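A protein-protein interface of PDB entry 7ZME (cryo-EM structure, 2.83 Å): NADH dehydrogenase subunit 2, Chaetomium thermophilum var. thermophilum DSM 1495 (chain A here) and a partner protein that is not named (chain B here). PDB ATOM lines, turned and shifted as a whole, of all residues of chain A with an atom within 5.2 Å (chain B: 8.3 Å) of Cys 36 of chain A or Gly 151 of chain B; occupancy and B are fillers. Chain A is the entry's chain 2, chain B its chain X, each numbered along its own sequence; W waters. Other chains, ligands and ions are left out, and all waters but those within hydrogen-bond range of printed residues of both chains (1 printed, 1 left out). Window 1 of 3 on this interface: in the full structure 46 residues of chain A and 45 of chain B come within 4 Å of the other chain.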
ATOM      1  N   MET A   1     -23.702 -15.903 -21.350  1.00  0.00           N
ATOM      2  CA  MET A   1     -22.731 -15.034 -20.696  1.00  0.00           C
ATOM      3  C   MET A   1     -23.372 -13.726 -20.237  1.00  0.00           C
ATOM      4  O   MET A   1     -23.016 -13.194 -19.191  1.00  0.00           O
ATOM      5  CB  MET A   1     -21.546 -14.746 -21.623  1.00  0.00           C
ATOM      6  CG  MET A   1     -20.504 -13.829 -21.006  1.00  0.00           C
ATOM      7  SD  MET A   1     -19.863 -14.488 -19.456  1.00  0.00           S
ATOM      8  CE  MET A   1     -18.832 -13.137 -18.909  1.00  0.00           C
ATOM      9  N   ILE A   2     -24.325 -13.211 -21.013  1.00  0.00           N
ATOM     10  CA  ILE A   2     -25.030 -12.006 -20.593  1.00  0.00           C
ATOM     11  C   ILE A   2     -25.848 -12.281 -19.337  1.00  0.00           C
ATOM     12  O   ILE A   2     -25.958 -11.424 -18.455  1.00  0.00           O
ATOM     13  CB  ILE A   2     -25.898 -11.450 -21.744  1.00  0.00           C
ATOM     14  CG1 ILE A   2     -26.446 -10.063 -21.397  1.00  0.00           C
ATOM     15  CG2 ILE A   2     -27.043 -12.380 -22.078  1.00  0.00           C
ATOM     16  CD1 ILE A   2     -25.427  -8.965 -21.434  1.00  0.00           C
ATOM     17  N   ALA A  32     -17.871  -7.386 -18.954  1.00  0.00           N
ATOM     18  CA  ALA A  32     -18.837  -8.478 -19.197  1.00  0.00           C
ATOM     19  C   ALA A  32     -19.338  -8.462 -20.645  1.00  0.00           C
ATOM     20  O   ALA A  32     -19.450  -9.550 -21.229  1.00  0.00           O
ATOM     21  CB  ALA A  32     -19.967  -8.349 -18.216  1.00  0.00           C
ATOM     22  N   LEU A  33     -19.633  -7.281 -21.197  1.00  0.00           N
ATOM     23  CA  LEU A  33     -20.153  -7.152 -22.581  1.00  0.00           C
ATOM     24  C   LEU A  33     -19.054  -7.473 -23.591  1.00  0.00           C
ATOM     25  O   LEU A  33     -19.398  -7.839 -24.722  1.00  0.00           O
ATOM     26  CB  LEU A  33     -20.730  -5.749 -22.770  1.00  0.00           C
ATOM     27  CG  LEU A  33     -22.106  -5.521 -22.155  1.00  0.00           C
ATOM     28  CD1 LEU A  33     -22.508  -4.065 -22.286  1.00  0.00           C
ATOM     29  CD2 LEU A  33     -23.134  -6.419 -22.815  1.00  0.00           C
ATOM     30  N   ALA A  34     -17.788  -7.379 -23.179  1.00  0.00           N
ATOM     31  CA  ALA A  34     -16.646  -7.708 -24.061  1.00  0.00           C
ATOM     32  C   ALA A  34     -16.499  -9.227 -24.127  1.00  0.00           C
ATOM     33  O   ALA A  34     -16.063  -9.721 -25.176  1.00  0.00           O
ATOM     34  CB  ALA A  34     -15.400  -7.100 -23.499  1.00  0.00           C
ATOM     35  N   TYR A  35     -16.903  -9.967 -23.091  1.00  0.00           N
ATOM     36  CA  TYR A  35     -16.843 -11.449 -23.159  1.00  0.00           C
ATOM     37  C   TYR A  35     -17.955 -11.956 -24.060  1.00  0.00           C
ATOM     38  O   TYR A  35     -17.740 -12.920 -24.800  1.00  0.00           O
ATOM     39  CB  TYR A  35     -16.903 -12.097 -21.778  1.00  0.00           C
ATOM     40  CG  TYR A  35     -15.617 -12.069 -20.997  1.00  0.00           C
ATOM     41  CD1 TYR A  35     -14.564 -12.903 -21.327  1.00  0.00           C
ATOM     42  CD2 TYR A  35     -15.462 -11.220 -19.918  1.00  0.00           C
ATOM     43  CE1 TYR A  35     -13.383 -12.886 -20.607  1.00  0.00           C
ATOM     44  CE2 TYR A  35     -14.286 -11.186 -19.192  1.00  0.00           C
ATOM     45  CZ  TYR A  35     -13.243 -12.020 -19.539  1.00  0.00           C
ATOM     46  OH  TYR A  35     -12.088 -11.983 -18.820  1.00  0.00           O
ATOM     47  N   CYS A  36     -19.094 -11.279 -24.024  1.00  0.00           N
ATOM     48  CA  CYS A  36     -20.226 -11.650 -24.901  1.00  0.00           C
ATOM     49  C   CYS A  36     -19.797 -11.482 -26.360  1.00  0.00           C
ATOM     50  O   CYS A  36     -20.197 -12.313 -27.181  1.00  0.00           O
ATOM     51  CB  CYS A  36     -21.433 -10.775 -24.588  1.00  0.00           C
ATOM     52  SG  CYS A  36     -22.062 -10.932 -22.899  1.00  0.00           S
ATOM     53  N   ILE A  37     -19.042 -10.428 -26.669  1.00  0.00           N
ATOM     54  CA  ILE A  37     -18.527 -10.203 -28.049  1.00  0.00           C
ATOM     55  C   ILE A  37     -17.568 -11.332 -28.452  1.00  0.00           C
ATOM     56  O   ILE A  37     -17.665 -11.788 -29.595  1.00  0.00           O
ATOM     57  CB  ILE A  37     -17.886  -8.805 -28.154  1.00  0.00           C
ATOM     58  CG1 ILE A  37     -18.949  -7.706 -28.122  1.00  0.00           C
ATOM     59  CG2 ILE A  37     -17.014  -8.686 -29.394  1.00  0.00           C
ATOM     60  CD1 ILE A  37     -18.435  -6.366 -27.673  1.00  0.00           C
ATOM     61  N   LEU A  38     -16.684 -11.762 -27.552  1.00  0.00           N
ATOM     62  CA  LEU A  38     -15.705 -12.832 -27.863  1.00  0.00           C
ATOM     63  C   LEU A  38     -16.466 -14.121 -28.159  1.00  0.00           C
ATOM     64  O   LEU A  38     -16.121 -14.793 -29.141  1.00  0.00           O
ATOM     65  CB  LEU A  38     -14.804 -13.022 -26.642  1.00  0.00           C
ATOM     66  CG  LEU A  38     -13.598 -13.935 -26.830  1.00  0.00           C
ATOM     67  CD1 LEU A  38     -12.663 -13.374 -27.889  1.00  0.00           C
ATOM     68  CD2 LEU A  38     -12.858 -14.116 -25.515  1.00  0.00           C
ATOM     69  N   HIS A  39     -17.477 -14.426 -27.350  1.00  0.00           N
ATOM     70  CA  HIS A  39     -18.296 -15.638 -27.554  1.00  0.00           C
ATOM     71  C   HIS A  39     -19.039 -15.535 -28.880  1.00  0.00           C
ATOM     72  O   HIS A  39     -19.044 -16.528 -29.623  1.00  0.00           O
ATOM     73  CB  HIS A  39     -19.221 -15.789 -26.351  1.00  0.00           C
ATOM     74  CG  HIS A  39     -18.471 -15.996 -25.080  1.00  0.00           C
ATOM     75  ND1 HIS A  39     -18.944 -15.567 -23.860  1.00  0.00           N
ATOM     76  CD2 HIS A  39     -17.270 -16.562 -24.839  1.00  0.00           C
ATOM     77  CE1 HIS A  39     -18.071 -15.867 -22.922  1.00  0.00           C
ATOM     78  NE2 HIS A  39     -17.036 -16.476 -23.498  1.00  0.00           N
ATOM     79  N   ASP A  40     -19.632 -14.374 -29.169  1.00  0.00           N
ATOM     80  CA  ASP A  40     -20.409 -14.172 -30.421  1.00  0.00           C
ATOM     81  C   ASP A  40     -19.509 -14.217 -31.658  1.00  0.00           C
ATOM     82  O   ASP A  40     -19.980 -14.712 -32.689  1.00  0.00           O
ATOM     83  CB  ASP A  40     -21.366 -12.995 -30.321  1.00  0.00           C
ATOM     84  CG  ASP A  40     -22.759 -13.389 -29.862  1.00  0.00           C
ATOM     85  OD1 ASP A  40     -22.875 -14.375 -29.109  1.00  0.00           O
ATOM     86  OD2 ASP A  40     -23.716 -12.720 -30.280  1.00  0.00           O
ATOM     87  N   THR A  41     -18.291 -13.684 -31.579  1.00  0.00           N
ATOM     88  CA  THR A  41     -17.332 -13.768 -32.710  1.00  0.00           C
ATOM     89  C   THR A  41     -16.987 -15.233 -32.960  1.00  0.00           C
ATOM     90  O   THR A  41     -16.899 -15.617 -34.132  1.00  0.00           O
ATOM     91  CB  THR A  41     -16.079 -12.928 -32.447  1.00  0.00           C
ATOM     92  OG1 THR A  41     -16.488 -11.637 -32.002  1.00  0.00           O
ATOM     93  CG2 THR A  41     -15.213 -12.781 -33.677  1.00  0.00           C
ATOM     94  N   PHE A  72     -23.862  -5.194 -28.342  1.00  0.00           N
ATOM     95  CA  PHE A  72     -22.881  -5.284 -27.228  1.00  0.00           C
ATOM     96  C   PHE A  72     -21.840  -4.165 -27.306  1.00  0.00           C
ATOM     97  O   PHE A  72     -21.390  -3.726 -26.249  1.00  0.00           O
ATOM     98  CB  PHE A  72     -22.199  -6.654 -27.214  1.00  0.00           C
ATOM     99  CG  PHE A  72     -23.068  -7.866 -26.998  1.00  0.00           C
ATOM    100  CD1 PHE A  72     -24.176  -7.821 -26.169  1.00  0.00           C
ATOM    101  CD2 PHE A  72     -22.749  -9.070 -27.605  1.00  0.00           C
ATOM    102  CE1 PHE A  72     -24.960  -8.947 -25.973  1.00  0.00           C
ATOM    103  CE2 PHE A  72     -23.539 -10.192 -27.415  1.00  0.00           C
ATOM    104  CZ  PHE A  72     -24.641 -10.129 -26.597  1.00  0.00           C
ATOM    105  N   ILE B  81     -16.411 -13.026 -13.211  1.00  0.00           N
ATOM    106  CA  ILE B  81     -16.958 -12.809 -14.548  1.00  0.00           C
ATOM    107  C   ILE B  81     -15.916 -13.140 -15.608  1.00  0.00           C
ATOM    108  O   ILE B  81     -16.231 -13.739 -16.644  1.00  0.00           O
ATOM    109  CB  ILE B  81     -17.486 -11.367 -14.681  1.00  0.00           C
ATOM    110  CG1 ILE B  81     -18.880 -11.259 -14.061  1.00  0.00           C
ATOM    111  CG2 ILE B  81     -17.518 -10.914 -16.136  1.00  0.00           C
ATOM    112  CD1 ILE B  81     -19.502  -9.899 -14.187  1.00  0.00           C
ATOM    113  N   GLY B  85     -16.412 -16.191 -18.150  1.00  0.00           N
ATOM    114  CA  GLY B  85     -16.290 -16.016 -19.585  1.00  0.00           C
ATOM    115  C   GLY B  85     -15.063 -16.689 -20.158  1.00  0.00           C
ATOM    116  O   GLY B  85     -15.039 -17.033 -21.343  1.00  0.00           O
ATOM    117  N   LEU B  88     -16.167 -20.360 -20.668  1.00  0.00           N
ATOM    118  CA  LEU B  88     -17.053 -20.425 -21.823  1.00  0.00           C
ATOM    119  C   LEU B  88     -16.262 -20.297 -23.113  1.00  0.00           C
ATOM    120  O   LEU B  88     -16.598 -20.923 -24.121  1.00  0.00           O
ATOM    121  CB  LEU B  88     -18.121 -19.336 -21.738  1.00  0.00           C
ATOM    122  CG  LEU B  88     -19.250 -19.541 -20.728  1.00  0.00           C
ATOM    123  CD1 LEU B  88     -20.069 -18.273 -20.591  1.00  0.00           C
ATOM    124  CD2 LEU B  88     -20.135 -20.712 -21.119  1.00  0.00           C
ATOM    125  N   GLN B  92     -15.888 -23.318 -25.929  1.00  0.00           N
ATOM    126  CA  GLN B  92     -16.292 -23.038 -27.332  1.00  0.00           C
ATOM    127  C   GLN B  92     -15.203 -23.456 -28.325  1.00  0.00           C
ATOM    128  O   GLN B  92     -15.562 -23.883 -29.426  1.00  0.00           O
ATOM    129  CB  GLN B  92     -16.619 -21.557 -27.490  1.00  0.00           C
ATOM    130  CG  GLN B  92     -18.079 -21.263 -27.785  1.00  0.00           C
ATOM    131  CD  GLN B  92     -18.339 -19.782 -27.674  1.00  0.00           C
ATOM    132  OE1 GLN B  92     -17.560 -19.044 -27.077  1.00  0.00           O
ATOM    133  NE2 GLN B  92     -19.443 -19.334 -28.248  1.00  0.00           N
ATOM    134  N   SER B 146     -25.576 -25.664 -29.212  1.00  0.00           N
ATOM    135  CA  SER B 146     -25.915 -24.686 -28.147  1.00  0.00           C
ATOM    136  C   SER B 146     -24.682 -23.889 -27.745  1.00  0.00           C
ATOM    137  O   SER B 146     -24.847 -22.901 -27.025  1.00  0.00           O
ATOM    138  CB  SER B 146     -26.536 -25.361 -26.958  1.00  0.00           C
ATOM    139  OG  SER B 146     -25.588 -26.156 -26.267  1.00  0.00           O
ATOM    140  N   ALA B 147     -23.475 -24.260 -28.145  1.00  0.00           N
ATOM    141  CA  ALA B 147     -22.297 -23.410 -27.835  1.00  0.00           C
ATOM    142  C   ALA B 147     -22.278 -22.137 -28.690  1.00  0.00           C
ATOM    143  O   ALA B 147     -21.539 -21.218 -28.345  1.00  0.00           O
ATOM    144  CB  ALA B 147     -21.025 -24.189 -27.924  1.00  0.00           C
ATOM    145  N   LEU B 148     -23.098 -22.078 -29.735  1.00  0.00           N
ATOM    146  CA  LEU B 148     -23.184 -20.906 -30.641  1.00  0.00           C
ATOM    147  C   LEU B 148     -24.042 -19.817 -29.994  1.00  0.00           C
ATOM    148  O   LEU B 148     -24.118 -18.721 -30.558  1.00  0.00           O
ATOM    149  CB  LEU B 148     -23.746 -21.376 -31.984  1.00  0.00           C
ATOM    150  CG  LEU B 148     -22.922 -22.452 -32.693  1.00  0.00           C
ATOM    151  CD1 LEU B 148     -23.693 -23.076 -33.841  1.00  0.00           C
ATOM    152  CD2 LEU B 148     -21.599 -21.895 -33.187  1.00  0.00           C
ATOM    153  N   PHE B 149     -24.671 -20.121 -28.858  1.00  0.00           N
ATOM    154  CA  PHE B 149     -25.469 -19.127 -28.089  1.00  0.00           C
ATOM    155  C   PHE B 149     -24.787 -18.831 -26.748  1.00  0.00           C
ATOM    156  O   PHE B 149     -25.414 -18.156 -25.937  1.00  0.00           O
ATOM    157  CB  PHE B 149     -26.905 -19.639 -27.951  1.00  0.00           C
ATOM    158  CG  PHE B 149     -27.981 -18.604 -27.741  1.00  0.00           C
ATOM    159  CD1 PHE B 149     -28.240 -17.644 -28.704  1.00  0.00           C
ATOM    160  CD2 PHE B 149     -28.767 -18.623 -26.603  1.00  0.00           C
ATOM    161  CE1 PHE B 149     -29.239 -16.702 -28.513  1.00  0.00           C
ATOM    162  CE2 PHE B 149     -29.767 -17.683 -26.415  1.00  0.00           C
ATOM    163  CZ  PHE B 149     -30.004 -16.725 -27.371  1.00  0.00           C
ATOM    164  N   PHE B 150     -23.538 -19.263 -26.552  1.00  0.00           N
ATOM    165  CA  PHE B 150     -22.787 -19.113 -25.264  1.00  0.00           C
ATOM    166  C   PHE B 150     -22.718 -17.673 -24.751  1.00  0.00           C
ATOM    167  O   PHE B 150     -22.683 -17.513 -23.528  1.00  0.00           O
ATOM    168  CB  PHE B 150     -21.396 -19.745 -25.357  1.00  0.00           C
ATOM    169  CG  PHE B 150     -21.320 -21.145 -24.817  1.00  0.00           C
ATOM    170  CD1 PHE B 150     -22.474 -21.841 -24.504  1.00  0.00           C
ATOM    171  CD2 PHE B 150     -20.097 -21.760 -24.613  1.00  0.00           C
ATOM    172  CE1 PHE B 150     -22.407 -23.126 -23.997  1.00  0.00           C
ATOM    173  CE2 PHE B 150     -20.033 -23.046 -24.106  1.00  0.00           C
ATOM    174  CZ  PHE B 150     -21.187 -23.727 -23.800  1.00  0.00           C
ATOM    175  N   GLY B 151     -22.641 -16.686 -25.650  1.00  0.00           N
ATOM    176  CA  GLY B 151     -22.582 -15.257 -25.286  1.00  0.00           C
ATOM    177  C   GLY B 151     -23.851 -14.804 -24.595  1.00  0.00           C
ATOM    178  O   GLY B 151     -23.793 -13.830 -23.837  1.00  0.00           O
ATOM    179  N   VAL B 152     -24.973 -15.448 -24.894  1.00  0.00           N
ATOM    180  CA  VAL B 152     -26.280 -15.027 -24.320  1.00  0.00           C
ATOM    181  C   VAL B 152     -26.682 -16.012 -23.224  1.00  0.00           C
ATOM    182  O   VAL B 152     -26.442 -15.717 -22.051  1.00  0.00           O
ATOM    183  CB  VAL B 152     -27.342 -14.975 -25.430  1.00  0.00           C
ATOM    184  CG1 VAL B 152     -28.599 -14.253 -24.975  1.00  0.00           C
ATOM    185  CG2 VAL B 152     -26.786 -14.348 -26.695  1.00  0.00           C
ATOM    186  N   MET B 153     -27.252 -17.147 -23.609  1.00  0.00           N
ATOM    187  CA  MET B 153     -27.635 -18.189 -22.633  1.00  0.00           C
ATOM    188  C   MET B 153     -26.659 -19.355 -22.794  1.00  0.00           C
ATOM    189  O   MET B 153     -26.527 -19.830 -23.920  1.00  0.00           O
ATOM    190  CB  MET B 153     -29.062 -18.687 -22.871  1.00  0.00           C
ATOM    191  CG  MET B 153     -29.405 -19.963 -22.131  1.00  0.00           C
ATOM    192  SD  MET B 153     -31.042 -20.582 -22.581  1.00  0.00           S
ATOM    193  CE  MET B 153     -32.063 -19.214 -22.043  1.00  0.00           C
ATOM    194  N   PRO B 154     -25.959 -19.841 -21.747  1.00  0.00           N
ATOM    195  CA  PRO B 154     -25.105 -21.018 -21.891  1.00  0.00           C
ATOM    196  C   PRO B 154     -25.850 -22.311 -21.593  1.00  0.00           C
ATOM    197  O   PRO B 154     -26.903 -22.329 -20.957  1.00  0.00           O
ATOM    198  CB  PRO B 154     -24.001 -20.772 -20.855  1.00  0.00           C
ATOM    199  CG  PRO B 154     -24.649 -19.913 -19.810  1.00  0.00           C
ATOM    200  CD  PRO B 154     -25.896 -19.288 -20.386  1.00  0.00           C
ATOM    201  N   TRP B 155     -25.273 -23.407 -22.077  1.00  0.00           N
ATOM    202  CA  TRP B 155     -25.850 -24.725 -21.869  1.00  0.00           C
ATOM    203  C   TRP B 155     -24.787 -25.773 -22.148  1.00  0.00           C
ATOM    204  O   TRP B 155     -23.941 -25.598 -23.027  1.00  0.00           O
ATOM    205  CB  TRP B 155     -27.072 -24.949 -22.763  1.00  0.00           C
ATOM    206  CG  TRP B 155     -27.974 -26.022 -22.264  1.00  0.00           C
ATOM    207  CD1 TRP B 155     -27.962 -27.330 -22.626  1.00  0.00           C
ATOM    208  CD2 TRP B 155     -29.021 -25.879 -21.300  1.00  0.00           C
ATOM    209  NE1 TRP B 155     -28.937 -28.017 -21.949  1.00  0.00           N
ATOM    210  CE2 TRP B 155     -29.602 -27.146 -21.127  1.00  0.00           C
ATOM    211  CE3 TRP B 155     -29.527 -24.802 -20.570  1.00  0.00           C
ATOM    212  CZ2 TRP B 155     -30.661 -27.367 -20.254  1.00  0.00           C
ATOM    213  CZ3 TRP B 155     -30.576 -25.022 -19.704  1.00  0.00           C
ATOM    214  CH2 TRP B 155     -31.133 -26.295 -19.554  1.00  0.00           C
HETATM  215  O   HOH W   1     -25.479 -15.827 -29.315  1.00  0.00           O
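NE2 of His 39 of chain A is in hydrogen-bond range of O of Gly 85 of chain B (3.0 Å). The side-chain amide nitrogen (NE2) of Gln 92 of chain B lies within hydrogen-bond range of the backbone carbonyl oxygen (O) of His 39 of chain A, at 3.2 Å. The backbone carbonyl oxygen of Phe 150 of chain B sits at hydrogen-bond distance from the backbone NH of Met 1 of chain A, 2.9 Å away. O of Gly 151 of chain B sits at hydrogen-bond distance from N of Met 1 of chain A (3.2 Å). The backbone carbonyl oxygen of Gly 151 of chain B is in hydrogen-bond range of the backbone NH of Ile 2 of chain A (2.9 Å). The backbone carbonyl oxygen (O) of Gly 151 of chain B is in hydrogen-bond range of the side-chain sulfur (SG) of Cys 36 of chain A, at 3.5 Å. The backbone NH of Met 1 of chain A lies within hydrogen-bond range of the backbone carbonyl oxygen of Val 152 of chain B, 2.8 Å away. N of Ile 2 of chain A sits close to O of Val 152 of chain B (3.4 Å).
Of the 14 printed residues of chain B, 7 touch a printed residue of chain A. Along chain B the printed residues that touch a printed residue of chain A span positions 81 to 152. Hydrophobic or aromatic side chains of chain A that line the printed part of chain B: Met 1, Ile 2, Tyr 35 and His 39. Along chain A the printed residues that touch a printed residue of chain B span positions 1 to 40.
Printed residues of chain B within 4 Å of Met 1 of chain A: Ile 81 (3.5 Å), Gly 85 (3.9 Å), Leu 88 (3.96 Å), Phe 150 (2.9 Å), Gly 151 (3.2 Å) and Val 152 (2.8 Å). Of the printed residues of chain B, Ile 2 of chain A touches Gly 151 (2.9 Å) and Val 152 (3.4 Å). Ala 32 of chain A touches none of the printed residues of chain B. Of the printed residues of chain B, Tyr 35 of chain A touches Gly 85 (3.96 Å). Cys 36 of chain A touches just one residue of chain B: Gly 151 (3.5 Å). Of the printed residues of chain A, Gln 92 of chain B touches His 39. Of chain A, only Met 1, Ile 2, Cys 36, His 39 and Asp 40 come within 4 Å of Gly 151 of chain B. Printed residues of chain A within 4 Å of Val 152 of chain B: Met 1 (2.8 Å) and Ile 2 (3.4 Å).
The side-chain amide nitrogen of Gln 92 of chain B lies within hydrogen-bond range of the backbone carbonyl oxygen of Ala 147 of chain B (2.8 Å). The backbone NH (N) of Ile 2 of chain A is in hydrogen-bond range of the side-chain sulfur (SG) of Cys 36 of chain A, 3.7 Å away. The side-chain sulfur (SG) of Cys 36 of chain A is in hydrogen-bond range of the backbone carbonyl oxygen (O) of Ala 32 of chain A (3.4 Å). O of Tyr 35 of chain A lies within hydrogen-bond range of ND1 of His 39 of chain A (3.1 Å).
Met 1 of chain A touches Ile 81 of chain B. Met 1 of chain A touches Gly 85 of chain B (SD to CA, 3.9 Å). Met 1 of chain A touches Leu 88 of chain B (SD to CD1, 3.96 Å). Gly 85 of chain B touches Tyr 35 of chain A. NE2 of His 39 of chain A touches CB of Leu 88 of chain B (3.5 Å). CA of Gly 151 of chain B touches CB of His 39 of chain A (3.6 Å). CA of Gly 151 of chain B touches OD1 of Asp 40 of chain A, at 3.9 Å.
Water W1 lies within hydrogen-bond range of the side-chain carboxylate (OD1) of Asp 40 of chain A (3.0 Å) and the backbone carbonyl oxygen (O) of Leu 148 of chain B (3.4 Å).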
